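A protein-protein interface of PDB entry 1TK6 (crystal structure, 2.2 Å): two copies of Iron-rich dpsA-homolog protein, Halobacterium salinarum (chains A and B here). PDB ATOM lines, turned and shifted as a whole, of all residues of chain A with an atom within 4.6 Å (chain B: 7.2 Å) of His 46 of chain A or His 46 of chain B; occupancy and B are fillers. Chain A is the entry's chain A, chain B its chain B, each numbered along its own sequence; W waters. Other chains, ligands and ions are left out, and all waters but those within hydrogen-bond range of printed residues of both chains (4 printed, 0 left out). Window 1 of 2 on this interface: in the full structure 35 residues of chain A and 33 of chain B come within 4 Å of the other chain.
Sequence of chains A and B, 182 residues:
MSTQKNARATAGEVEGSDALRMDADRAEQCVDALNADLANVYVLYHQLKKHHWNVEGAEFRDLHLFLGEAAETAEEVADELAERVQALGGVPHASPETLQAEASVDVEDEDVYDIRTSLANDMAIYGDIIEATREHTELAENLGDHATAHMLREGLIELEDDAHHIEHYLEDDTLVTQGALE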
ATOM      1  N   TYR A  42       5.762  23.636  15.711  1.00  0.00           N
ATOM      2  CA  TYR A  42       6.489  24.316  16.726  1.00  0.00           C
ATOM      3  C   TYR A  42       7.307  23.315  17.445  1.00  0.00           C
ATOM      4  O   TYR A  42       8.445  23.667  17.901  1.00  0.00           O
ATOM      5  CB  TYR A  42       5.658  25.186  17.675  1.00  0.00           C
ATOM      6  CG  TYR A  42       5.850  26.644  17.469  1.00  0.00           C
ATOM      7  CD1 TYR A  42       4.786  27.495  17.286  1.00  0.00           C
ATOM      8  CD2 TYR A  42       7.130  27.173  17.436  1.00  0.00           C
ATOM      9  CE1 TYR A  42       5.016  28.936  17.102  1.00  0.00           C
ATOM     10  CE2 TYR A  42       7.358  28.514  17.262  1.00  0.00           C
ATOM     11  CZ  TYR A  42       6.295  29.408  17.078  1.00  0.00           C
ATOM     12  OH  TYR A  42       6.645  30.747  16.875  1.00  0.00           O
ATOM     13  N   VAL A  43       6.833  22.060  17.587  1.00  0.00           N
ATOM     14  CA  VAL A  43       7.761  21.113  18.180  1.00  0.00           C
ATOM     15  C   VAL A  43       8.940  20.780  17.230  1.00  0.00           C
ATOM     16  O   VAL A  43      10.056  20.551  17.627  1.00  0.00           O
ATOM     17  CB  VAL A  43       7.093  19.867  18.793  1.00  0.00           C
ATOM     18  CG1 VAL A  43       5.727  20.078  19.373  1.00  0.00           C
ATOM     19  CG2 VAL A  43       7.121  18.826  17.964  1.00  0.00           C
ATOM     20  N   LEU A  44       8.675  20.746  15.955  1.00  0.00           N
ATOM     21  CA  LEU A  44       9.718  20.636  15.000  1.00  0.00           C
ATOM     22  C   LEU A  44      10.792  21.747  15.162  1.00  0.00           C
ATOM     23  O   LEU A  44      11.942  21.500  15.285  1.00  0.00           O
ATOM     24  CB  LEU A  44       9.142  20.700  13.604  1.00  0.00           C
ATOM     25  CG  LEU A  44      10.285  20.656  12.515  1.00  0.00           C
ATOM     26  CD1 LEU A  44      11.157  19.449  12.547  1.00  0.00           C
ATOM     27  CD2 LEU A  44       9.784  20.888  11.154  1.00  0.00           C
ATOM     28  N   TYR A  45      10.332  22.968  15.205  1.00  0.00           N
ATOM     29  CA  TYR A  45      11.205  24.123  15.403  1.00  0.00           C
ATOM     30  C   TYR A  45      12.070  23.950  16.619  1.00  0.00           C
ATOM     31  O   TYR A  45      13.287  24.070  16.553  1.00  0.00           O
ATOM     32  CB  TYR A  45      10.335  25.349  15.565  1.00  0.00           C
ATOM     33  CG  TYR A  45      11.046  26.511  16.148  1.00  0.00           C
ATOM     34  CD1 TYR A  45      11.775  27.393  15.346  1.00  0.00           C
ATOM     35  CD2 TYR A  45      10.917  26.786  17.475  1.00  0.00           C
ATOM     36  CE1 TYR A  45      12.403  28.459  15.879  1.00  0.00           C
ATOM     37  CE2 TYR A  45      11.518  27.833  18.029  1.00  0.00           C
ATOM     38  CZ  TYR A  45      12.218  28.701  17.197  1.00  0.00           C
ATOM     39  OH  TYR A  45      12.856  29.707  17.798  1.00  0.00           O
ATOM     40  N   HIS A  46      11.452  23.695  17.757  1.00  0.00           N
ATOM     41  CA  HIS A  46      12.237  23.569  19.008  1.00  0.00           C
ATOM     42  C   HIS A  46      13.277  22.429  18.997  1.00  0.00           C
ATOM     43  O   HIS A  46      14.367  22.529  19.584  1.00  0.00           O
ATOM     44  CB  HIS A  46      11.351  23.457  20.240  1.00  0.00           C
ATOM     45  CG  HIS A  46      10.834  24.771  20.693  1.00  0.00           C
ATOM     46  ND1 HIS A  46      11.660  25.708  21.240  1.00  0.00           N
ATOM     47  CD2 HIS A  46       9.563  25.248  20.822  1.00  0.00           C
ATOM     48  CE1 HIS A  46      10.939  26.789  21.520  1.00  0.00           C
ATOM     49  NE2 HIS A  46       9.661  26.514  21.331  1.00  0.00           N
ATOM     50  N   GLN A  47      12.978  21.375  18.296  1.00  0.00           N
ATOM     51  CA  GLN A  47      13.963  20.297  18.180  1.00  0.00           C
ATOM     52  C   GLN A  47      15.074  20.566  17.157  1.00  0.00           C
ATOM     53  O   GLN A  47      16.257  20.279  17.400  1.00  0.00           O
ATOM     54  CB  GLN A  47      13.264  18.989  17.862  1.00  0.00           C
ATOM     55  CG  GLN A  47      14.196  17.831  17.822  1.00  0.00           C
ATOM     56  CD  GLN A  47      13.479  16.501  18.121  1.00  0.00           C
ATOM     57  OE1 GLN A  47      12.917  16.325  19.224  1.00  0.00           O
ATOM     58  NE2 GLN A  47      13.462  15.596  17.121  1.00  0.00           N
ATOM     59  N   LEU A  48      14.736  21.179  16.072  1.00  0.00           N
ATOM     60  CA  LEU A  48      15.761  21.647  15.194  1.00  0.00           C
ATOM     61  C   LEU A  48      16.666  22.625  15.912  1.00  0.00           C
ATOM     62  O   LEU A  48      17.879  22.575  15.748  1.00  0.00           O
ATOM     63  CB  LEU A  48      15.150  22.348  13.969  1.00  0.00           C
ATOM     64  CG  LEU A  48      14.337  21.481  12.992  1.00  0.00           C
ATOM     65  CD1 LEU A  48      13.700  22.294  12.014  1.00  0.00           C
ATOM     66  CD2 LEU A  48      15.306  20.486  12.294  1.00  0.00           C
ATOM     67  N   LYS A  49      16.100  23.536  16.695  1.00  0.00           N
ATOM     68  CA  LYS A  49      16.956  24.457  17.475  1.00  0.00           C
ATOM     69  C   LYS A  49      17.939  23.645  18.353  1.00  0.00           C
ATOM     70  O   LYS A  49      19.149  23.879  18.407  1.00  0.00           O
ATOM     71  CB  LYS A  49      16.127  25.361  18.387  1.00  0.00           C
ATOM     72  CG  LYS A  49      15.283  26.366  17.692  1.00  0.00           C
ATOM     73  CD  LYS A  49      16.060  27.328  16.747  1.00  0.00           C
ATOM     74  CE  LYS A  49      16.904  28.233  17.355  1.00  0.00           C
ATOM     75  NZ  LYS A  49      16.726  29.463  16.613  1.00  0.00           N
ATOM     76  N   LYS A  50      17.346  22.716  19.093  1.00  0.00           N
ATOM     77  CA  LYS A  50      18.145  21.846  19.941  1.00  0.00           C
ATOM     78  C   LYS A  50      19.309  21.270  19.151  1.00  0.00           C
ATOM     79  O   LYS A  50      20.477  21.269  19.639  1.00  0.00           O
ATOM     80  CB  LYS A  50      17.219  20.697  20.582  1.00  0.00           C
ATOM     81  CG  LYS A  50      18.093  19.722  21.408  1.00  0.00           C
ATOM     82  CD  LYS A  50      17.357  18.405  21.670  1.00  0.00           C
ATOM     83  CE  LYS A  50      18.042  17.487  22.676  1.00  0.00           C
ATOM     84  NZ  LYS A  50      17.108  16.314  22.960  1.00  0.00           N
ATOM     85  N   ALA A  94      -0.696  28.370  21.576  1.00  0.00           N
ATOM     86  CA  ALA A  94       0.195  29.425  21.862  1.00  0.00           C
ATOM     87  C   ALA A  94       1.296  28.987  22.822  1.00  0.00           C
ATOM     88  O   ALA A  94       2.451  29.067  22.461  1.00  0.00           O
ATOM     89  CB  ALA A  94      -0.624  30.550  22.457  1.00  0.00           C
ATOM     90  N   PRO A  96       3.987  26.953  25.062  1.00  0.00           N
ATOM     91  CA  PRO A  96       4.821  25.796  24.765  1.00  0.00           C
ATOM     92  C   PRO A  96       4.230  24.502  25.267  1.00  0.00           C
ATOM     93  O   PRO A  96       4.172  23.509  24.498  1.00  0.00           O
ATOM     94  CB  PRO A  96       6.148  26.117  25.478  1.00  0.00           C
ATOM     95  CG  PRO A  96       6.181  27.513  25.677  1.00  0.00           C
ATOM     96  CD  PRO A  96       4.744  28.041  25.678  1.00  0.00           C
ATOM     97  N   LEU A  99       1.474  23.570  22.822  1.00  0.00           N
ATOM     98  CA  LEU A  99       1.975  23.212  21.558  1.00  0.00           C
ATOM     99  C   LEU A  99       2.438  21.785  21.626  1.00  0.00           C
ATOM    100  O   LEU A  99       2.049  20.986  20.794  1.00  0.00           O
ATOM    101  CB  LEU A  99       3.110  24.193  21.146  1.00  0.00           C
ATOM    102  CG  LEU A  99       2.603  25.551  20.747  1.00  0.00           C
ATOM    103  CD1 LEU A  99       3.722  26.525  20.624  1.00  0.00           C
ATOM    104  CD2 LEU A  99       1.789  25.526  19.511  1.00  0.00           C
ATOM    105  N   ASN B  40      12.646  31.148  30.581  1.00  0.00           N
ATOM    106  CA  ASN B  40      11.822  32.358  30.672  1.00  0.00           C
ATOM    107  C   ASN B  40      11.678  33.095  29.321  1.00  0.00           C
ATOM    108  O   ASN B  40      10.569  33.520  28.931  1.00  0.00           O
ATOM    109  CB  ASN B  40      12.442  33.234  31.742  1.00  0.00           C
ATOM    110  CG  ASN B  40      12.019  32.790  33.151  1.00  0.00           C
ATOM    111  OD1 ASN B  40      11.014  32.111  33.320  1.00  0.00           O
ATOM    112  ND2 ASN B  40      12.746  33.172  34.115  1.00  0.00           N
ATOM    113  N   VAL B  41      12.780  33.223  28.609  1.00  0.00           N
ATOM    114  CA  VAL B  41      12.810  34.068  27.406  1.00  0.00           C
ATOM    115  C   VAL B  41      12.050  33.309  26.334  1.00  0.00           C
ATOM    116  O   VAL B  41      11.437  33.944  25.511  1.00  0.00           O
ATOM    117  CB  VAL B  41      14.189  34.362  26.948  1.00  0.00           C
ATOM    118  CG1 VAL B  41      14.160  35.115  25.673  1.00  0.00           C
ATOM    119  CG2 VAL B  41      14.985  35.213  27.982  1.00  0.00           C
ATOM    120  N   TYR B  42      12.010  31.947  26.364  1.00  0.00           N
ATOM    121  CA  TYR B  42      11.293  31.253  25.340  1.00  0.00           C
ATOM    122  C   TYR B  42       9.873  31.190  25.615  1.00  0.00           C
ATOM    123  O   TYR B  42       9.128  31.210  24.671  1.00  0.00           O
ATOM    124  CB  TYR B  42      11.789  29.892  25.076  1.00  0.00           C
ATOM    125  CG  TYR B  42      12.424  29.733  23.726  1.00  0.00           C
ATOM    126  CD1 TYR B  42      13.588  29.039  23.572  1.00  0.00           C
ATOM    127  CD2 TYR B  42      11.834  30.233  22.571  1.00  0.00           C
ATOM    128  CE1 TYR B  42      14.169  28.830  22.327  1.00  0.00           C
ATOM    129  CE2 TYR B  42      12.416  30.059  21.337  1.00  0.00           C
ATOM    130  CZ  TYR B  42      13.572  29.332  21.233  1.00  0.00           C
ATOM    131  OH  TYR B  42      14.158  29.152  20.024  1.00  0.00           O
ATOM    132  N   VAL B  43       9.444  31.199  26.890  1.00  0.00           N
ATOM    133  CA  VAL B  43       8.023  31.472  27.169  1.00  0.00           C
ATOM    134  C   VAL B  43       7.637  32.873  26.780  1.00  0.00           C
ATOM    135  O   VAL B  43       6.601  33.056  26.171  1.00  0.00           O
ATOM    136  CB  VAL B  43       7.426  30.996  28.525  1.00  0.00           C
ATOM    137  CG1 VAL B  43       8.073  29.794  29.116  1.00  0.00           C
ATOM    138  CG2 VAL B  43       7.133  32.056  29.423  1.00  0.00           C
ATOM    139  N   LEU B  44       8.501  33.838  27.005  1.00  0.00           N
ATOM    140  CA  LEU B  44       8.281  35.174  26.526  1.00  0.00           C
ATOM    141  C   LEU B  44       8.025  35.242  25.008  1.00  0.00           C
ATOM    142  O   LEU B  44       6.988  35.805  24.533  1.00  0.00           O
ATOM    143  CB  LEU B  44       9.448  36.093  26.829  1.00  0.00           C
ATOM    144  CG  LEU B  44       9.246  37.475  26.287  1.00  0.00           C
ATOM    145  CD1 LEU B  44       8.042  38.249  26.852  1.00  0.00           C
ATOM    146  CD2 LEU B  44      10.462  38.296  26.526  1.00  0.00           C
ATOM    147  N   TYR B  45       8.895  34.591  24.296  1.00  0.00           N
ATOM    148  CA  TYR B  45       8.804  34.491  22.882  1.00  0.00           C
ATOM    149  C   TYR B  45       7.477  33.974  22.449  1.00  0.00           C
ATOM    150  O   TYR B  45       6.827  34.560  21.590  1.00  0.00           O
ATOM    151  CB  TYR B  45       9.913  33.628  22.346  1.00  0.00           C
ATOM    152  CG  TYR B  45       9.698  33.161  20.941  1.00  0.00           C
ATOM    153  CD1 TYR B  45       9.997  33.981  19.844  1.00  0.00           C
ATOM    154  CD2 TYR B  45       9.243  31.883  20.730  1.00  0.00           C
ATOM    155  CE1 TYR B  45       9.801  33.554  18.583  1.00  0.00           C
ATOM    156  CE2 TYR B  45       9.086  31.382  19.503  1.00  0.00           C
ATOM    157  CZ  TYR B  45       9.365  32.209  18.433  1.00  0.00           C
ATOM    158  OH  TYR B  45       9.063  31.668  17.253  1.00  0.00           O
ATOM    159  N   HIS B  46       7.041  32.934  23.096  1.00  0.00           N
ATOM    160  CA  HIS B  46       5.860  32.280  22.677  1.00  0.00           C
ATOM    161  C   HIS B  46       4.623  33.078  22.988  1.00  0.00           C
ATOM    162  O   HIS B  46       3.732  33.039  22.170  1.00  0.00           O
ATOM    163  CB  HIS B  46       5.757  30.842  23.195  1.00  0.00           C
ATOM    164  CG  HIS B  46       6.485  29.805  22.385  1.00  0.00           C
ATOM    165  ND1 HIS B  46       5.839  28.868  21.683  1.00  0.00           N
ATOM    166  CD2 HIS B  46       7.764  29.587  22.080  1.00  0.00           C
ATOM    167  CE1 HIS B  46       6.653  28.026  21.084  1.00  0.00           C
ATOM    168  NE2 HIS B  46       7.840  28.409  21.343  1.00  0.00           N
ATOM    169  N   GLN B  47       4.615  33.798  24.119  1.00  0.00           N
ATOM    170  CA  GLN B  47       3.547  34.689  24.506  1.00  0.00           C
ATOM    171  C   GLN B  47       3.534  35.994  23.632  1.00  0.00           C
ATOM    172  O   GLN B  47       2.464  36.489  23.281  1.00  0.00           O
ATOM    173  CB  GLN B  47       3.621  35.023  26.048  1.00  0.00           C
ATOM    174  CG  GLN B  47       2.474  35.937  26.505  1.00  0.00           C
ATOM    175  CD  GLN B  47       1.958  35.628  27.902  1.00  0.00           C
ATOM    176  OE1 GLN B  47       1.633  34.481  28.204  1.00  0.00           O
ATOM    177  NE2 GLN B  47       2.030  36.626  28.799  1.00  0.00           N
ATOM    178  N   LEU B  48       4.704  36.531  23.280  1.00  0.00           N
ATOM    179  CA  LEU B  48       4.705  37.637  22.347  1.00  0.00           C
ATOM    180  C   LEU B  48       4.169  37.186  21.013  1.00  0.00           C
ATOM    181  O   LEU B  48       3.503  37.955  20.372  1.00  0.00           O
ATOM    182  CB  LEU B  48       6.075  38.234  22.163  1.00  0.00           C
ATOM    183  CG  LEU B  48       6.689  38.751  23.406  1.00  0.00           C
ATOM    184  CD1 LEU B  48       8.152  38.962  23.261  1.00  0.00           C
ATOM    185  CD2 LEU B  48       5.975  40.093  23.786  1.00  0.00           C
ATOM    186  N   LYS B  49       4.477  35.976  20.569  1.00  0.00           N
ATOM    187  CA  LYS B  49       3.887  35.491  19.315  1.00  0.00           C
ATOM    188  C   LYS B  49       2.355  35.371  19.389  1.00  0.00           C
ATOM    189  O   LYS B  49       1.675  35.739  18.484  1.00  0.00           O
ATOM    190  CB  LYS B  49       4.444  34.140  18.934  1.00  0.00           C
ATOM    191  CG  LYS B  49       5.907  34.235  18.595  1.00  0.00           C
ATOM    192  CD  LYS B  49       6.208  34.951  17.260  1.00  0.00           C
ATOM    193  CE  LYS B  49       5.794  34.252  16.170  1.00  0.00           C
ATOM    194  NZ  LYS B  49       6.755  34.556  14.873  1.00  0.00           N
ATOM    195  N   LYS B  50       1.861  34.819  20.467  1.00  0.00           N
ATOM    196  CA  LYS B  50       0.416  34.792  20.727  1.00  0.00           C
ATOM    197  C   LYS B  50      -0.231  36.132  20.546  1.00  0.00           C
ATOM    198  O   LYS B  50      -1.249  36.262  19.844  1.00  0.00           O
ATOM    199  CB  LYS B  50       0.154  34.318  22.151  1.00  0.00           C
ATOM    200  CG  LYS B  50      -1.296  34.091  22.440  1.00  0.00           C
ATOM    201  CD  LYS B  50      -1.503  33.818  23.925  1.00  0.00           C
ATOM    202  CE  LYS B  50      -2.983  33.858  24.267  1.00  0.00           C
ATOM    203  NZ  LYS B  50      -3.211  33.319  25.609  1.00  0.00           N
ATOM    204  N   HIS B  51       0.317  37.137  21.202  1.00  0.00           N
ATOM    205  CA  HIS B  51      -0.237  38.475  21.238  1.00  0.00           C
ATOM    206  C   HIS B  51      -0.154  39.115  19.910  1.00  0.00           C
ATOM    207  O   HIS B  51      -1.103  39.773  19.488  1.00  0.00           O
ATOM    208  CB  HIS B  51       0.454  39.284  22.369  1.00  0.00           C
ATOM    209  CG  HIS B  51       0.113  38.801  23.710  1.00  0.00           C
ATOM    210  ND1 HIS B  51       0.888  39.030  24.821  1.00  0.00           N
ATOM    211  CD2 HIS B  51      -0.899  38.001  24.114  1.00  0.00           C
ATOM    212  CE1 HIS B  51       0.333  38.431  25.845  1.00  0.00           C
ATOM    213  NE2 HIS B  51      -0.768  37.838  25.459  1.00  0.00           N
ATOM    214  N   HIS B  52       0.945  38.837  19.202  1.00  0.00           N
ATOM    215  CA  HIS B  52       1.169  39.319  17.847  1.00  0.00           C
ATOM    216  C   HIS B  52       0.167  38.689  16.942  1.00  0.00           C
ATOM    217  O   HIS B  52      -0.328  39.374  15.989  1.00  0.00           O
ATOM    218  CB  HIS B  52       2.537  38.801  17.470  1.00  0.00           C
ATOM    219  CG  HIS B  52       2.850  38.746  16.025  1.00  0.00           C
ATOM    220  ND1 HIS B  52       3.480  39.772  15.376  1.00  0.00           N
ATOM    221  CD2 HIS B  52       2.716  37.750  15.111  1.00  0.00           C
ATOM    222  CE1 HIS B  52       3.720  39.418  14.111  1.00  0.00           C
ATOM    223  NE2 HIS B  52       3.262  38.200  13.928  1.00  0.00           N
ATOM    224  N   TRP B  53      -0.067  37.392  17.090  1.00  0.00           N
ATOM    225  CA  TRP B  53      -1.092  36.735  16.250  1.00  0.00           C
ATOM    226  C   TRP B  53      -2.447  37.224  16.490  1.00  0.00           C
ATOM    227  O   TRP B  53      -3.183  37.308  15.575  1.00  0.00           O
ATOM    228  CB  TRP B  53      -1.164  35.233  16.485  1.00  0.00           C
ATOM    229  CG  TRP B  53       0.103  34.534  16.163  1.00  0.00           C
ATOM    230  CD1 TRP B  53       1.010  34.893  15.117  1.00  0.00           C
ATOM    231  CD2 TRP B  53       0.632  33.345  16.727  1.00  0.00           C
ATOM    232  NE1 TRP B  53       2.062  34.001  15.080  1.00  0.00           N
ATOM    233  CE2 TRP B  53       1.876  33.061  16.054  1.00  0.00           C
ATOM    234  CE3 TRP B  53       0.252  32.512  17.726  1.00  0.00           C
ATOM    235  CZ2 TRP B  53       2.652  31.991  16.369  1.00  0.00           C
ATOM    236  CZ3 TRP B  53       1.038  31.413  18.056  1.00  0.00           C
ATOM    237  CH2 TRP B  53       2.199  31.144  17.360  1.00  0.00           C
ATOM    238  N   ALA B  71       9.117  39.549  19.591  1.00  0.00           N
ATOM    239  CA  ALA B  71       9.273  38.099  19.544  1.00  0.00           C
ATOM    240  C   ALA B  71      10.577  37.697  18.879  1.00  0.00           C
ATOM    241  O   ALA B  71      11.248  36.822  19.391  1.00  0.00           O
ATOM    242  CB  ALA B  71       8.185  37.454  18.819  1.00  0.00           C
ATOM    243  N   ALA B  74      13.379  38.363  21.408  1.00  0.00           N
ATOM    244  CA  ALA B  74      13.423  37.270  22.426  1.00  0.00           C
ATOM    245  C   ALA B  74      14.061  36.017  21.826  1.00  0.00           C
ATOM    246  O   ALA B  74      14.747  35.271  22.485  1.00  0.00           O
ATOM    247  CB  ALA B  74      12.079  36.915  22.955  1.00  0.00           C
ATOM    248  N   HIS B  93      17.867  23.783  27.688  1.00  0.00           N
ATOM    249  CA  HIS B  93      16.510  23.247  27.753  1.00  0.00           C
ATOM    250  C   HIS B  93      15.935  23.462  26.386  1.00  0.00           C
ATOM    251  O   HIS B  93      16.106  24.592  25.821  1.00  0.00           O
ATOM    252  CB  HIS B  93      15.614  24.068  28.638  1.00  0.00           C
ATOM    253  CG  HIS B  93      16.041  24.141  30.054  1.00  0.00           C
ATOM    254  ND1 HIS B  93      16.549  23.054  30.732  1.00  0.00           N
ATOM    255  CD2 HIS B  93      15.996  25.161  30.942  1.00  0.00           C
ATOM    256  CE1 HIS B  93      16.769  23.412  31.986  1.00  0.00           C
ATOM    257  NE2 HIS B  93      16.470  24.675  32.127  1.00  0.00           N
ATOM    258  N   ALA B  94      15.354  22.391  25.814  1.00  0.00           N
ATOM    259  CA  ALA B  94      15.051  22.369  24.421  1.00  0.00           C
ATOM    260  C   ALA B  94      13.530  22.155  24.153  1.00  0.00           C
ATOM    261  O   ALA B  94      12.893  22.884  23.376  1.00  0.00           O
ATOM    262  CB  ALA B  94      15.868  21.292  23.785  1.00  0.00           C
ATOM    263  N   SER B  95      12.897  21.175  24.768  1.00  0.00           N
ATOM    264  CA  SER B  95      11.525  20.910  24.286  1.00  0.00           C
ATOM    265  C   SER B  95      10.623  21.948  24.835  1.00  0.00           C
ATOM    266  O   SER B  95      10.929  22.614  25.826  1.00  0.00           O
ATOM    267  CB  SER B  95      11.066  19.511  24.687  1.00  0.00           C
ATOM    268  OG  SER B  95      10.741  19.525  26.054  1.00  0.00           O
ATOM    269  N   PRO B  96       9.530  22.184  24.190  1.00  0.00           N
ATOM    270  CA  PRO B  96       8.599  23.232  24.649  1.00  0.00           C
ATOM    271  C   PRO B  96       8.023  22.940  26.050  1.00  0.00           C
ATOM    272  O   PRO B  96       8.042  23.864  26.867  1.00  0.00           O
ATOM    273  CB  PRO B  96       7.531  23.306  23.532  1.00  0.00           C
ATOM    274  CG  PRO B  96       7.963  22.431  22.408  1.00  0.00           C
ATOM    275  CD  PRO B  96       9.128  21.575  22.932  1.00  0.00           C
ATOM    276  N   GLU B  97       7.633  21.697  26.375  1.00  0.00           N
ATOM    277  CA  GLU B  97       7.181  21.415  27.759  1.00  0.00           C
ATOM    278  C   GLU B  97       8.316  21.564  28.757  1.00  0.00           C
ATOM    279  O   GLU B  97       8.092  22.075  29.803  1.00  0.00           O
ATOM    280  CB  GLU B  97       6.563  20.021  27.932  1.00  0.00           C
ATOM    281  CG  GLU B  97       7.344  19.126  28.969  1.00  0.00           C
ATOM    282  CD  GLU B  97       7.547  17.711  28.486  1.00  0.00           C
ATOM    283  OE1 GLU B  97       8.602  17.514  27.718  1.00  0.00           O
ATOM    284  OE2 GLU B  97       6.652  16.813  28.907  1.00  0.00           O
ATOM    285  N   LEU B  99      10.770  23.819  28.403  1.00  0.00           N
ATOM    286  CA  LEU B  99      10.931  25.268  28.566  1.00  0.00           C
ATOM    287  C   LEU B  99       9.919  25.866  29.530  1.00  0.00           C
ATOM    288  O   LEU B  99      10.204  26.708  30.338  1.00  0.00           O
ATOM    289  CB  LEU B  99      10.797  25.951  27.231  1.00  0.00           C
ATOM    290  CG  LEU B  99      11.976  25.671  26.264  1.00  0.00           C
ATOM    291  CD1 LEU B  99      11.739  26.031  24.807  1.00  0.00           C
ATOM    292  CD2 LEU B  99      13.288  26.339  26.705  1.00  0.00           C
ATOM    293  N   GLN B 100       8.705  25.509  29.355  1.00  0.00           N
ATOM    294  CA  GLN B 100       7.635  26.089  30.157  1.00  0.00           C
ATOM    295  C   GLN B 100       7.718  25.577  31.582  1.00  0.00           C
ATOM    296  O   GLN B 100       7.590  26.352  32.499  1.00  0.00           O
ATOM    297  CB  GLN B 100       6.218  25.783  29.593  1.00  0.00           C
ATOM    298  CG  GLN B 100       5.115  26.583  30.402  1.00  0.00           C
ATOM    299  CD  GLN B 100       3.772  26.688  29.637  1.00  0.00           C
ATOM    300  OE1 GLN B 100       3.731  26.490  28.404  1.00  0.00           O
ATOM    301  NE2 GLN B 100       2.679  26.968  30.372  1.00  0.00           N
HETATM  302  O   HOH W   1      14.085  24.466  21.742  1.00  0.00           O
HETATM  303  O   HOH W   2       3.391  30.640  20.654  1.00  0.00           O
HETATM  304  O   HOH W   3      16.408  30.656  19.698  1.00  0.00           O
HETATM  305  O   HOH W   4       6.278  31.718  14.460  1.00  0.00           O
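Water W1 bridges O of Ala 94 of chain B (2.6 Å) and ND1 of His 46 of chain A (2.8 Å).
Water W2 bridges O of Ala 94 of chain A (2.6 Å) and O of His 46 of chain B (2.9 Å).
Water W4 lies within hydrogen-bond range of the side-chain hydroxyl of Tyr 42 of chain A and the side-chain amino group of Lys 49 of chain B.
Tyr 42 of chain A touches His 46 of chain B, and with the chains exchanged His 46 of chain A touches Tyr 42 of chain B.
Lys 50 of chain A touches Ala 94 of chain B, and with the chains exchanged Ala 94 of chain A touches Lys 50 of chain B.
Printed residues of chain B within 4 Å of Lys 50 of chain A: Ala 94 (3.5 Å).
Printed residues of chain B within 4 Å of Ala 94 of chain A: His 46 and Lys 50.
Printed residues of chain B within 4 Å of Pro 96 of chain A: His 46, Pro 96 and Gln 100.
Of chain A, only Tyr 42 (3.8 Å), His 46 (2.6 Å), Ala 94 (3.5 Å), Pro 96 (3.9 Å) and Leu 99 (3.3 Å) come within 4 Å of His 46 of chain B.
Of the printed residues of chain A, Lys 50 of chain B touches Ala 94 (3.6 Å).
The nearest printed residue of chain B that does not touch Tyr 42 of chain A is Pro 96 of chain B (4.7 Å).
The side-chain hydroxyl (OH) of Tyr 45 of chain A is in hydrogen-bond range of the side-chain hydroxyl (OH) of Tyr 42 of chain B (2.6 Å).
The side-chain hydroxyl (OH) of Tyr 42 of chain A lies within hydrogen-bond range of the side-chain hydroxyl (OH) of Tyr 45 of chain B (2.6 Å).
A ring nitrogen (ND1) of His 46 of chain B lies within hydrogen-bond range of the backbone carbonyl oxygen (O) of Ala 94 of chain A (3.5 Å).
N of Pro 96 of chain A lies close to OE1 of Gln 100 of chain B (3.4 Å).
A ring nitrogen (NE2) of His 46 of chain A is in hydrogen-bond range of a ring nitrogen (NE2) of His 46 of chain B (2.6 Å).
Printed residues of chain A that touch a printed residue of chain B: Tyr 42, Tyr 45, His 46, Lys 49, Lys 50, Ala 94, Pro 96 and Leu 99.
Hydrophobic or aromatic side chains of chain A within 4 Å of the printed part of chain B: Tyr 42, Tyr 45, His 46, Ala 94, Pro 96 and Leu 99.
Among the printed residues, 18 pairs touch across the chains.
Among the printed residues, no Asp or Glu carboxylate lies within 4 Å of a Lys or Arg side-chain nitrogen of the other chain.
Among the printed residues, merely in contact across the chains: Pro 96 of chain A with Pro 96 of chain B, Leu 99 of chain A with His 46 of chain B, His 46 of chain A with Leu 99 of chain B, Lys 50 of chain A with Ala 94 of chain B, His 46 of chain A with Ala 94 of chain B, Tyr 42 of chain A with Trp 53 of chain B, His 46 of chain A with Tyr 42 of chain B, Ala 94 of chain A with Lys 50 of chain B, His 46 of chain A with Pro 96 of chain B, Tyr 42 of chain A with Lys 49 of chain B, Tyr 42 of chain A with His 46 of chain B, Lys 49 of chain A with Tyr 42 of chain B and Pro 96 of chain A with His 46 of chain B.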
